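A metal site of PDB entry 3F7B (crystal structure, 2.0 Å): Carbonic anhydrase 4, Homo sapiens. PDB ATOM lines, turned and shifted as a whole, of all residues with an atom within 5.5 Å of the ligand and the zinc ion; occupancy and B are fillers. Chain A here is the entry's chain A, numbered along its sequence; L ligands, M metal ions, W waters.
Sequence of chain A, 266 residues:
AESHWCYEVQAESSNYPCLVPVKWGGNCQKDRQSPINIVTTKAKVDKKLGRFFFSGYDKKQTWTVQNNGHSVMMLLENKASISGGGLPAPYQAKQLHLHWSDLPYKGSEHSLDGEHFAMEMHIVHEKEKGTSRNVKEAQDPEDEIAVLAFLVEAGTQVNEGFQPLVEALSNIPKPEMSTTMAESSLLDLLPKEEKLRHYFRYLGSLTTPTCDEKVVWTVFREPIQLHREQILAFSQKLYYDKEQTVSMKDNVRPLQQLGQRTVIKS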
ATOM      1  N   TRP A   5      -4.269   4.738  13.262  1.00  0.00           N
ATOM      2  CA  TRP A   5      -5.526   3.957  13.140  1.00  0.00           C
ATOM      3  C   TRP A   5      -6.213   3.874  14.492  1.00  0.00           C
ATOM      4  O   TRP A   5      -5.559   3.917  15.555  1.00  0.00           O
ATOM      5  CB  TRP A   5      -5.251   2.599  12.515  1.00  0.00           C
ATOM      6  CG  TRP A   5      -4.560   1.605  13.391  1.00  0.00           C
ATOM      7  CD1 TRP A   5      -3.193   1.318  13.535  1.00  0.00           C
ATOM      8  CD2 TRP A   5      -5.245   0.709  14.256  1.00  0.00           C
ATOM      9  NE1 TRP A   5      -3.026   0.242  14.446  1.00  0.00           N
ATOM     10  CE2 TRP A   5      -4.279  -0.124  14.876  1.00  0.00           C
ATOM     11  CE3 TRP A   5      -6.608   0.476  14.489  1.00  0.00           C
ATOM     12  CZ2 TRP A   5      -4.649  -1.157  15.757  1.00  0.00           C
ATOM     13  CZ3 TRP A   5      -6.973  -0.581  15.373  1.00  0.00           C
ATOM     14  CH2 TRP A   5      -5.992  -1.368  15.970  1.00  0.00           C
ATOM     15  N   TYR A   7     -10.328   2.316  16.181  1.00  0.00           N
ATOM     16  CA  TYR A   7     -11.690   1.708  15.954  1.00  0.00           C
ATOM     17  C   TYR A   7     -12.673   2.871  16.067  1.00  0.00           C
ATOM     18  O   TYR A   7     -12.406   3.945  16.640  1.00  0.00           O
ATOM     19  CB  TYR A   7     -12.024   0.731  17.059  1.00  0.00           C
ATOM     20  CG  TYR A   7     -11.142  -0.486  17.015  1.00  0.00           C
ATOM     21  CD1 TYR A   7     -11.300  -1.445  15.985  1.00  0.00           C
ATOM     22  CD2 TYR A   7     -10.163  -0.705  18.005  1.00  0.00           C
ATOM     23  CE1 TYR A   7     -10.489  -2.575  15.939  1.00  0.00           C
ATOM     24  CE2 TYR A   7      -9.347  -1.859  17.962  1.00  0.00           C
ATOM     25  CZ  TYR A   7      -9.524  -2.793  16.927  1.00  0.00           C
ATOM     26  OH  TYR A   7      -8.677  -3.957  16.809  1.00  0.00           O
ATOM     27  N   ASN A  68      -1.861  -2.665  24.736  1.00  0.00           N
ATOM     28  CA  ASN A  68      -1.103  -1.970  23.699  1.00  0.00           C
ATOM     29  C   ASN A  68      -1.948  -0.845  23.159  1.00  0.00           C
ATOM     30  O   ASN A  68      -1.745  -0.450  22.055  1.00  0.00           O
ATOM     31  CB  ASN A  68      -0.681  -2.957  22.559  1.00  0.00           C
ATOM     32  CG  ASN A  68      -1.885  -3.651  21.860  1.00  0.00           C
ATOM     33  OD1 ASN A  68      -3.062  -3.328  22.135  1.00  0.00           O
ATOM     34  ND2 ASN A  68      -1.596  -4.584  20.923  1.00  0.00           N
ATOM     35  N   HIS A  70      -4.953  -1.187  21.989  1.00  0.00           N
ATOM     36  CA  HIS A  70      -6.018  -1.694  21.094  1.00  0.00           C
ATOM     37  C   HIS A  70      -6.684  -2.956  21.669  1.00  0.00           C
ATOM     38  O   HIS A  70      -7.811  -3.332  21.259  1.00  0.00           O
ATOM     39  CB  HIS A  70      -5.416  -2.105  19.731  1.00  0.00           C
ATOM     40  CG  HIS A  70      -4.460  -1.103  19.175  1.00  0.00           C
ATOM     41  ND1 HIS A  70      -4.872   0.142  18.742  1.00  0.00           N
ATOM     42  CD2 HIS A  70      -3.121  -1.164  18.977  1.00  0.00           C
ATOM     43  CE1 HIS A  70      -3.811   0.817  18.297  1.00  0.00           C
ATOM     44  NE2 HIS A  70      -2.736   0.050  18.429  1.00  0.00           N
ATOM     45  N   SER A  71      -5.989  -3.629  22.561  1.00  0.00           N
ATOM     46  CA  SER A  71      -6.483  -4.922  23.069  1.00  0.00           C
ATOM     47  C   SER A  71      -5.645  -5.292  24.279  1.00  0.00           C
ATOM     48  O   SER A  71      -4.721  -4.564  24.678  1.00  0.00           O
ATOM     49  CB  SER A  71      -6.301  -6.043  22.017  1.00  0.00           C
ATOM     50  OG  SER A  71      -6.744  -7.268  22.561  1.00  0.00           O
ATOM     51  N   MET A  73      -2.978  -8.164  25.224  1.00  0.00           N
ATOM     52  CA  MET A  73      -2.246  -9.168  24.494  1.00  0.00           C
ATOM     53  C   MET A  73      -1.272  -9.952  25.374  1.00  0.00           C
ATOM     54  O   MET A  73      -0.382  -9.381  26.043  1.00  0.00           O
ATOM     55  CB  MET A  73      -1.433  -8.466  23.338  1.00  0.00           C
ATOM     56  CG  MET A  73      -0.552  -9.418  22.559  1.00  0.00           C
ATOM     57  SD  MET A  73       0.361  -8.588  21.243  1.00  0.00           S
ATOM     58  CE  MET A  73      -0.949  -7.855  20.227  1.00  0.00           C
ATOM     59  N   LYS A  94       2.549 -17.016  18.681  1.00  0.00           N
ATOM     60  CA  LYS A  94       3.255 -15.744  18.890  1.00  0.00           C
ATOM     61  C   LYS A  94       2.616 -14.898  20.000  1.00  0.00           C
ATOM     62  O   LYS A  94       3.315 -14.287  20.812  1.00  0.00           O
ATOM     63  CB  LYS A  94       3.289 -14.890  17.561  1.00  0.00           C
ATOM     64  CG  LYS A  94       4.064 -15.550  16.374  1.00  0.00           C
ATOM     65  CD  LYS A  94       5.590 -15.668  16.754  1.00  0.00           C
ATOM     66  CE  LYS A  94       6.203 -16.763  15.858  1.00  0.00           C
ATOM     67  NZ  LYS A  94       7.701 -16.761  15.877  1.00  0.00           N
ATOM     68  N   GLN A  95       1.269 -14.755  19.968  1.00  0.00           N
ATOM     69  CA  GLN A  95       0.600 -13.851  20.932  1.00  0.00           C
ATOM     70  C   GLN A  95      -0.867 -14.235  20.956  1.00  0.00           C
ATOM     71  O   GLN A  95      -1.329 -14.823  19.969  1.00  0.00           O
ATOM     72  CB  GLN A  95       0.794 -12.399  20.506  1.00  0.00           C
ATOM     73  CG  GLN A  95       0.452 -12.087  19.017  1.00  0.00           C
ATOM     74  CD  GLN A  95      -0.785 -11.229  18.781  1.00  0.00           C
ATOM     75  OE1 GLN A  95      -1.727 -11.121  19.604  1.00  0.00           O
ATOM     76  NE2 GLN A  95      -0.786 -10.587  17.647  1.00  0.00           N
ATOM     77  N   HIS A  97      -4.725 -12.371  21.783  1.00  0.00           N
ATOM     78  CA  HIS A  97      -5.386 -11.149  22.263  1.00  0.00           C
ATOM     79  C   HIS A  97      -6.905 -11.379  22.109  1.00  0.00           C
ATOM     80  O   HIS A  97      -7.356 -12.424  21.632  1.00  0.00           O
ATOM     81  CB  HIS A  97      -4.920  -9.898  21.494  1.00  0.00           C
ATOM     82  CG  HIS A  97      -5.146 -10.013  19.982  1.00  0.00           C
ATOM     83  ND1 HIS A  97      -4.238 -10.619  19.134  1.00  0.00           N
ATOM     84  CD2 HIS A  97      -6.232  -9.733  19.213  1.00  0.00           C
ATOM     85  CE1 HIS A  97      -4.730 -10.670  17.902  1.00  0.00           C
ATOM     86  NE2 HIS A  97      -5.941 -10.118  17.922  1.00  0.00           N
ATOM     87  N   LEU A  98      -7.687 -10.391  22.496  1.00  0.00           N
ATOM     88  CA  LEU A  98      -9.152 -10.531  22.365  1.00  0.00           C
ATOM     89  C   LEU A  98      -9.805  -9.282  21.823  1.00  0.00           C
ATOM     90  O   LEU A  98      -9.196  -8.176  21.862  1.00  0.00           O
ATOM     91  CB  LEU A  98      -9.751 -10.906  23.774  1.00  0.00           C
ATOM     92  CG  LEU A  98      -9.303 -12.305  24.307  1.00  0.00           C
ATOM     93  CD1 LEU A  98      -8.161 -12.151  25.243  1.00  0.00           C
ATOM     94  CD2 LEU A  98     -10.526 -13.042  24.981  1.00  0.00           C
ATOM     95  N   HIS A  99     -11.049  -9.439  21.367  1.00  0.00           N
ATOM     96  CA  HIS A  99     -11.859  -8.340  20.911  1.00  0.00           C
ATOM     97  C   HIS A  99     -13.155  -8.489  21.700  1.00  0.00           C
ATOM     98  O   HIS A  99     -13.570  -9.643  21.961  1.00  0.00           O
ATOM     99  CB  HIS A  99     -12.178  -8.484  19.382  1.00  0.00           C
ATOM    100  CG  HIS A  99     -10.918  -8.467  18.524  1.00  0.00           C
ATOM    101  ND1 HIS A  99     -10.357  -7.275  18.077  1.00  0.00           N
ATOM    102  CD2 HIS A  99     -10.062  -9.449  18.174  1.00  0.00           C
ATOM    103  CE1 HIS A  99      -9.226  -7.546  17.422  1.00  0.00           C
ATOM    104  NE2 HIS A  99      -9.054  -8.855  17.416  1.00  0.00           N
ATOM    105  N   GLU A 109     -15.503 -10.455  16.206  1.00  0.00           N
ATOM    106  CA  GLU A 109     -15.272  -9.912  14.860  1.00  0.00           C
ATOM    107  C   GLU A 109     -16.011 -10.723  13.767  1.00  0.00           C
ATOM    108  O   GLU A 109     -16.700 -10.167  12.863  1.00  0.00           O
ATOM    109  CB  GLU A 109     -13.768  -9.856  14.585  1.00  0.00           C
ATOM    110  CG  GLU A 109     -13.149  -8.782  15.539  1.00  0.00           C
ATOM    111  CD  GLU A 109     -11.819  -8.181  14.931  1.00  0.00           C
ATOM    112  OE1 GLU A 109     -10.955  -9.024  14.614  1.00  0.00           O
ATOM    113  OE2 GLU A 109     -11.604  -6.932  14.909  1.00  0.00           O
ATOM    114  N   HIS A 122      -8.224 -14.415  19.701  1.00  0.00           N
ATOM    115  CA  HIS A 122      -7.390 -14.763  18.547  1.00  0.00           C
ATOM    116  C   HIS A 122      -6.032 -15.239  19.019  1.00  0.00           C
ATOM    117  O   HIS A 122      -5.364 -14.498  19.734  1.00  0.00           O
ATOM    118  CB  HIS A 122      -7.168 -13.524  17.674  1.00  0.00           C
ATOM    119  CG  HIS A 122      -8.387 -13.132  16.901  1.00  0.00           C
ATOM    120  ND1 HIS A 122      -8.597 -11.842  16.435  1.00  0.00           N
ATOM    121  CD2 HIS A 122      -9.472 -13.852  16.530  1.00  0.00           C
ATOM    122  CE1 HIS A 122      -9.743 -11.796  15.783  1.00  0.00           C
ATOM    123  NE2 HIS A 122     -10.305 -12.981  15.863  1.00  0.00           N
ATOM    124  N   VAL A 124      -2.595 -16.111  17.669  1.00  0.00           N
ATOM    125  CA  VAL A 124      -1.857 -15.861  16.412  1.00  0.00           C
ATOM    126  C   VAL A 124      -0.593 -16.744  16.361  1.00  0.00           C
ATOM    127  O   VAL A 124       0.237 -16.692  17.309  1.00  0.00           O
ATOM    128  CB  VAL A 124      -1.455 -14.359  16.349  1.00  0.00           C
ATOM    129  CG1 VAL A 124      -0.668 -14.074  15.017  1.00  0.00           C
ATOM    130  CG2 VAL A 124      -2.759 -13.459  16.475  1.00  0.00           C
ATOM    131  N   HIS A 125      -0.427 -17.528  15.285  1.00  0.00           N
ATOM    132  CA  HIS A 125       0.714 -18.438  15.135  1.00  0.00           C
ATOM    133  C   HIS A 125       1.397 -18.150  13.785  1.00  0.00           C
ATOM    134  O   HIS A 125       0.754 -17.647  12.880  1.00  0.00           O
ATOM    135  CB  HIS A 125       0.321 -19.928  15.053  1.00  0.00           C
ATOM    136  CG  HIS A 125      -0.467 -20.415  16.219  1.00  0.00           C
ATOM    137  ND1 HIS A 125      -1.678 -19.865  16.576  1.00  0.00           N
ATOM    138  CD2 HIS A 125      -0.159 -21.322  17.156  1.00  0.00           C
ATOM    139  CE1 HIS A 125      -2.115 -20.466  17.677  1.00  0.00           C
ATOM    140  NE2 HIS A 125      -1.223 -21.357  18.043  1.00  0.00           N
ATOM    141  N   GLU A 126       2.675 -18.519  13.663  1.00  0.00           N
ATOM    142  CA  GLU A 126       3.404 -18.279  12.412  1.00  0.00           C
ATOM    143  C   GLU A 126       3.969 -19.574  11.855  1.00  0.00           C
ATOM    144  O   GLU A 126       4.514 -20.400  12.605  1.00  0.00           O
ATOM    145  CB  GLU A 126       4.490 -17.210  12.646  1.00  0.00           C
ATOM    146  CG  GLU A 126       5.541 -17.160  11.567  1.00  0.00           C
ATOM    147  CD  GLU A 126       6.164 -15.772  11.446  1.00  0.00           C
ATOM    148  OE1 GLU A 126       7.112 -15.479  12.236  1.00  0.00           O
ATOM    149  OE2 GLU A 126       5.690 -14.994  10.581  1.00  0.00           O
ATOM    150  N   ILE A 145       0.378 -17.035   8.434  1.00  0.00           N
ATOM    151  CA  ILE A 145      -0.078 -16.811   9.817  1.00  0.00           C
ATOM    152  C   ILE A 145      -1.359 -17.652  10.004  1.00  0.00           C
ATOM    153  O   ILE A 145      -2.220 -17.681   9.136  1.00  0.00           O
ATOM    154  CB  ILE A 145      -0.333 -15.273  10.080  1.00  0.00           C
ATOM    155  CG1 ILE A 145       1.014 -14.525  10.163  1.00  0.00           C
ATOM    156  CG2 ILE A 145      -1.042 -15.029  11.489  1.00  0.00           C
ATOM    157  CD1 ILE A 145       0.839 -13.234   9.519  1.00  0.00           C
ATOM    158  N   VAL A 147      -4.391 -18.070  12.563  1.00  0.00           N
ATOM    159  CA  VAL A 147      -5.057 -17.486  13.742  1.00  0.00           C
ATOM    160  C   VAL A 147      -6.181 -18.436  14.156  1.00  0.00           C
ATOM    161  O   VAL A 147      -6.925 -18.923  13.285  1.00  0.00           O
ATOM    162  CB  VAL A 147      -5.571 -16.077  13.461  1.00  0.00           C
ATOM    163  CG1 VAL A 147      -6.334 -15.536  14.735  1.00  0.00           C
ATOM    164  CG2 VAL A 147      -4.387 -15.129  13.123  1.00  0.00           C
ATOM    165  N   SER A 205      -7.129 -11.946   6.148  1.00  0.00           N
ATOM    166  CA  SER A 205      -6.127 -11.016   6.531  1.00  0.00           C
ATOM    167  C   SER A 205      -6.034 -10.903   8.060  1.00  0.00           C
ATOM    168  O   SER A 205      -6.936 -11.383   8.752  1.00  0.00           O
ATOM    169  CB  SER A 205      -6.519  -9.636   5.946  1.00  0.00           C
ATOM    170  OG  SER A 205      -7.569  -9.009   6.656  1.00  0.00           O
ATOM    171  N   LEU A 206      -4.980 -10.227   8.561  1.00  0.00           N
ATOM    172  CA  LEU A 206      -5.031  -9.582   9.889  1.00  0.00           C
ATOM    173  C   LEU A 206      -6.169  -8.579   9.933  1.00  0.00           C
ATOM    174  O   LEU A 206      -6.502  -7.963   8.890  1.00  0.00           O
ATOM    175  CB  LEU A 206      -3.671  -8.880  10.185  1.00  0.00           C
ATOM    176  CG  LEU A 206      -2.569  -9.946  10.011  1.00  0.00           C
ATOM    177  CD1 LEU A 206      -1.241  -9.286  10.165  1.00  0.00           C
ATOM    178  CD2 LEU A 206      -2.771 -10.970  11.069  1.00  0.00           C
ATOM    179  N   THR A 207      -6.771  -8.395  11.121  1.00  0.00           N
ATOM    180  CA  THR A 207      -7.877  -7.482  11.278  1.00  0.00           C
ATOM    181  C   THR A 207      -7.477  -6.162  11.874  1.00  0.00           C
ATOM    182  O   THR A 207      -8.363  -5.370  12.264  1.00  0.00           O
ATOM    183  CB  THR A 207      -9.038  -8.079  12.094  1.00  0.00           C
ATOM    184  OG1 THR A 207      -8.628  -8.341  13.451  1.00  0.00           O
ATOM    185  CG2 THR A 207      -9.455  -9.477  11.466  1.00  0.00           C
ATOM    186  N   THR A 208      -6.166  -5.893  11.960  1.00  0.00           N
ATOM    187  CA  THR A 208      -5.794  -4.475  12.229  1.00  0.00           C
ATOM    188  C   THR A 208      -4.699  -4.116  11.190  1.00  0.00           C
ATOM    189  O   THR A 208      -4.126  -5.004  10.584  1.00  0.00           O
ATOM    190  CB  THR A 208      -5.152  -4.369  13.597  1.00  0.00           C
ATOM    191  OG1 THR A 208      -4.080  -5.313  13.639  1.00  0.00           O
ATOM    192  CG2 THR A 208      -6.081  -4.838  14.712  1.00  0.00           C
ATOM    193  N   PRO A 209      -4.440  -2.810  10.959  1.00  0.00           N
ATOM    194  CA  PRO A 209      -3.365  -2.424   9.970  1.00  0.00           C
ATOM    195  C   PRO A 209      -2.124  -3.172  10.293  1.00  0.00           C
ATOM    196  O   PRO A 209      -1.793  -3.286  11.453  1.00  0.00           O
ATOM    197  CB  PRO A 209      -3.156  -0.900  10.195  1.00  0.00           C
ATOM    198  CG  PRO A 209      -4.683  -0.440  10.686  1.00  0.00           C
ATOM    199  CD  PRO A 209      -5.123  -1.647  11.552  1.00  0.00           C
ATOM    200  N   LYS A 214      -2.216 -12.540   4.658  1.00  0.00           N
ATOM    201  CA  LYS A 214      -1.423 -13.762   4.770  1.00  0.00           C
ATOM    202  C   LYS A 214      -1.938 -14.710   5.853  1.00  0.00           C
ATOM    203  O   LYS A 214      -1.165 -15.452   6.429  1.00  0.00           O
ATOM    204  CB  LYS A 214       0.042 -13.394   5.076  1.00  0.00           C
ATOM    205  CG  LYS A 214       0.211 -12.294   6.076  1.00  0.00           C
ATOM    206  CD  LYS A 214       1.772 -11.957   6.301  1.00  0.00           C
ATOM    207  CE  LYS A 214       1.958 -11.002   7.477  1.00  0.00           C
ATOM    208  NZ  LYS A 214       3.347 -10.630   7.956  1.00  0.00           N
ATOM    209  N   VAL A 215      -3.242 -14.640   6.159  1.00  0.00           N
ATOM    210  CA  VAL A 215      -3.772 -15.462   7.233  1.00  0.00           C
ATOM    211  C   VAL A 215      -4.584 -16.635   6.738  1.00  0.00           C
ATOM    212  O   VAL A 215      -5.563 -16.461   5.960  1.00  0.00           O
ATOM    213  CB  VAL A 215      -4.634 -14.612   8.250  1.00  0.00           C
ATOM    214  CG1 VAL A 215      -5.160 -15.488   9.402  1.00  0.00           C
ATOM    215  CG2 VAL A 215      -3.769 -13.468   8.852  1.00  0.00           C
ATOM    216  N   TRP A 217      -7.371 -18.683   8.377  1.00  0.00           N
ATOM    217  CA  TRP A 217      -8.265 -18.452   9.485  1.00  0.00           C
ATOM    218  C   TRP A 217      -8.831 -19.784   9.921  1.00  0.00           C
ATOM    219  O   TRP A 217      -9.178 -20.636   9.060  1.00  0.00           O
ATOM    220  CB  TRP A 217      -9.462 -17.426   9.223  1.00  0.00           C
ATOM    221  CG  TRP A 217      -8.999 -15.966   9.438  1.00  0.00           C
ATOM    222  CD1 TRP A 217      -8.487 -15.112   8.459  1.00  0.00           C
ATOM    223  CD2 TRP A 217      -8.900 -15.221  10.690  1.00  0.00           C
ATOM    224  NE1 TRP A 217      -8.133 -13.884   9.021  1.00  0.00           N
ATOM    225  CE2 TRP A 217      -8.326 -13.952  10.395  1.00  0.00           C
ATOM    226  CE3 TRP A 217      -9.189 -15.538  12.026  1.00  0.00           C
ATOM    227  CZ2 TRP A 217      -8.080 -13.008  11.360  1.00  0.00           C
ATOM    228  CZ3 TRP A 217      -8.992 -14.547  13.011  1.00  0.00           C
ATOM    229  CH2 TRP A 217      -8.424 -13.320  12.688  1.00  0.00           C
HETATM  230  O1  LIG L   1      -0.625  -7.353  16.455  1.00  0.00           O
HETATM  231  C1  LIG L   1      -1.703  -7.303  15.827  1.00  0.00           C
HETATM  232  N1  LIG L   1      -2.328  -6.104  15.586  1.00  0.00           N
HETATM  233  C2  LIG L   1      -1.829  -4.786  16.101  1.00  0.00           C
HETATM  234  C3  LIG L   1      -2.175  -4.605  17.586  1.00  0.00           C
HETATM  235  C4  LIG L   1      -3.536  -5.202  17.972  1.00  0.00           C
HETATM  236  C5  LIG L   1      -3.567  -6.465  18.426  1.00  0.00           C
HETATM  237  C6  LIG L   1      -4.723  -7.037  18.751  1.00  0.00           C
HETATM  238  C7  LIG L   1      -5.918  -6.423  18.613  1.00  0.00           C
HETATM  239  C8  LIG L   1      -5.945  -5.123  18.185  1.00  0.00           C
HETATM  240  C9  LIG L   1      -4.725  -4.533  17.867  1.00  0.00           C
HETATM  241  C10 LIG L   1      -2.296  -8.584  15.244  1.00  0.00           C
HETATM  242  C11 LIG L   1      -3.649  -8.781  15.014  1.00  0.00           C
HETATM  243  C12 LIG L   1      -1.363  -9.550  14.828  1.00  0.00           C
HETATM  244  N2  LIG L   1      -1.756 -10.669  14.301  1.00  0.00           N
HETATM  245  C13 LIG L   1      -3.044 -10.914  14.129  1.00  0.00           C
HETATM  246  C14 LIG L   1      -4.004  -9.994  14.512  1.00  0.00           C
HETATM  247  S1  LIG L   1      -5.703 -10.461  14.222  1.00  0.00           S
HETATM  248  O2  LIG L   1      -5.841 -10.356  12.779  1.00  0.00           O
HETATM  249  O3  LIG L   1      -5.871 -11.740  14.861  1.00  0.00           O
HETATM  250  N3  LIG L   1      -6.698  -9.305  14.972  1.00  0.00           N
HETATM  251  S2  LIG L   1       0.382  -9.227  15.016  1.00  0.00           S
HETATM  252  C15 LIG L   1       1.277 -10.562  14.342  1.00  0.00           C
HETATM  253  C16 LIG L   1       1.211 -10.776  12.952  1.00  0.00           C
HETATM  254  C17 LIG L   1       1.955 -11.808  12.409  1.00  0.00           C
HETATM  255  C18 LIG L   1       2.740 -12.621  13.243  1.00  0.00           C
HETATM  256  C19 LIG L   1       2.787 -12.396  14.622  1.00  0.00           C
HETATM  257  C20 LIG L   1       2.068 -11.346  15.198  1.00  0.00           C
HETATM  258 ZN    ZN M   1      -7.533 -10.059  16.669  1.00  0.00          ZN
HETATM  259  O   HOH W   1      -0.494  -1.648  15.864  1.00  0.00           O
HETATM  260  O   HOH W   2       1.441  -6.634  17.781  1.00  0.00           O
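The backbone NH of Thr 207 lies within hydrogen-bond range of an oxygen (O2) of the ligand, 2.7 Å away.
OG1 of Thr 207 lies close to N3 of the ligand (2.6 Å).
N1 of the ligand lies within hydrogen-bond range of OG1 of Thr 208, at 2.7 Å.
The side-chain amide nitrogen (NE2) of Gln 95 lies close to a sulfur (S2) of the ligand (3.2 Å).
ND1 of His 97 sits at hydrogen-bond distance from OE1 of Gln 95, 2.6 Å away.
The side-chain hydroxyl (OG1) of Thr 207 is in hydrogen-bond range of the side-chain carboxylate (OE1) of Glu 109 (2.7 Å).
The side-chain amide oxygen of Gln 95 lies close to the side-chain sulfur of Met 73 (3.7 Å).
N of His 70 is in hydrogen-bond range of OD1 of Asn 68, 2.9 Å away.
The side-chain amide oxygen of Asn 68 lies within hydrogen-bond range of the backbone NH of Ser 71 (3.0 Å).
The side-chain hydroxyl of Ser 71 is in hydrogen-bond range of the backbone carbonyl oxygen of Leu 98.
O of Val 124 sits at hydrogen-bond distance from N of Lys 94, 2.7 Å away.
The side-chain carboxylate of Glu 126 is in salt-bridge range of the side-chain amino group of Lys 94 (3.9 Å).
Trp 5 touches the ligand.
OH of Tyr 7 touches C8 of the ligand (3.3 Å).
ND2 of Asn 68 touches C3 of the ligand, 3.4 Å away.
His 70 touches the ligand (CB to C9, 3.1 Å).
Ser 71 touches the ligand.
Met 73 touches the ligand (CE to C5, 3.5 Å).
Lys 94 touches the ligand (CG to C19, 3.8 Å).
Val 124 touches the ligand.
Ile 145 touches the ligand.
CG1 of Val 147 touches O3 of the ligand, 3.8 Å away.
CD2 of Leu 206 touches C13 of the ligand, at 3.1 Å.
Trp 217 touches the ligand (CH2 to O3, 3.7 Å).
Hydrophobic or aromatic side chains within 4 Å of the ligand: Trp 5, His 70, Met 73, His 97, His 99, His 122, Val 124, Ile 145, Val 147, Leu 206 and Trp 217.
The nearest printed residue that does not touch the ligand is Glu 109 (4.3 Å).
The zinc ion is bound by a ring nitrogen (NE2) of His 97 (2.0 Å), a nitrogen (N3) of the ligand (2.0 Å), a ring nitrogen (NE2) of His 99 (2.1 Å) and a ring nitrogen (ND1) of His 122 (2.1 Å).
The zinc ion has four donor atoms within binding distance.
Thr 207 touches the zinc ion (OG1 to ZN, 3.8 Å).
The nearest printed residue that does not touch the zinc ion is Glu 109 (4.1 Å).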
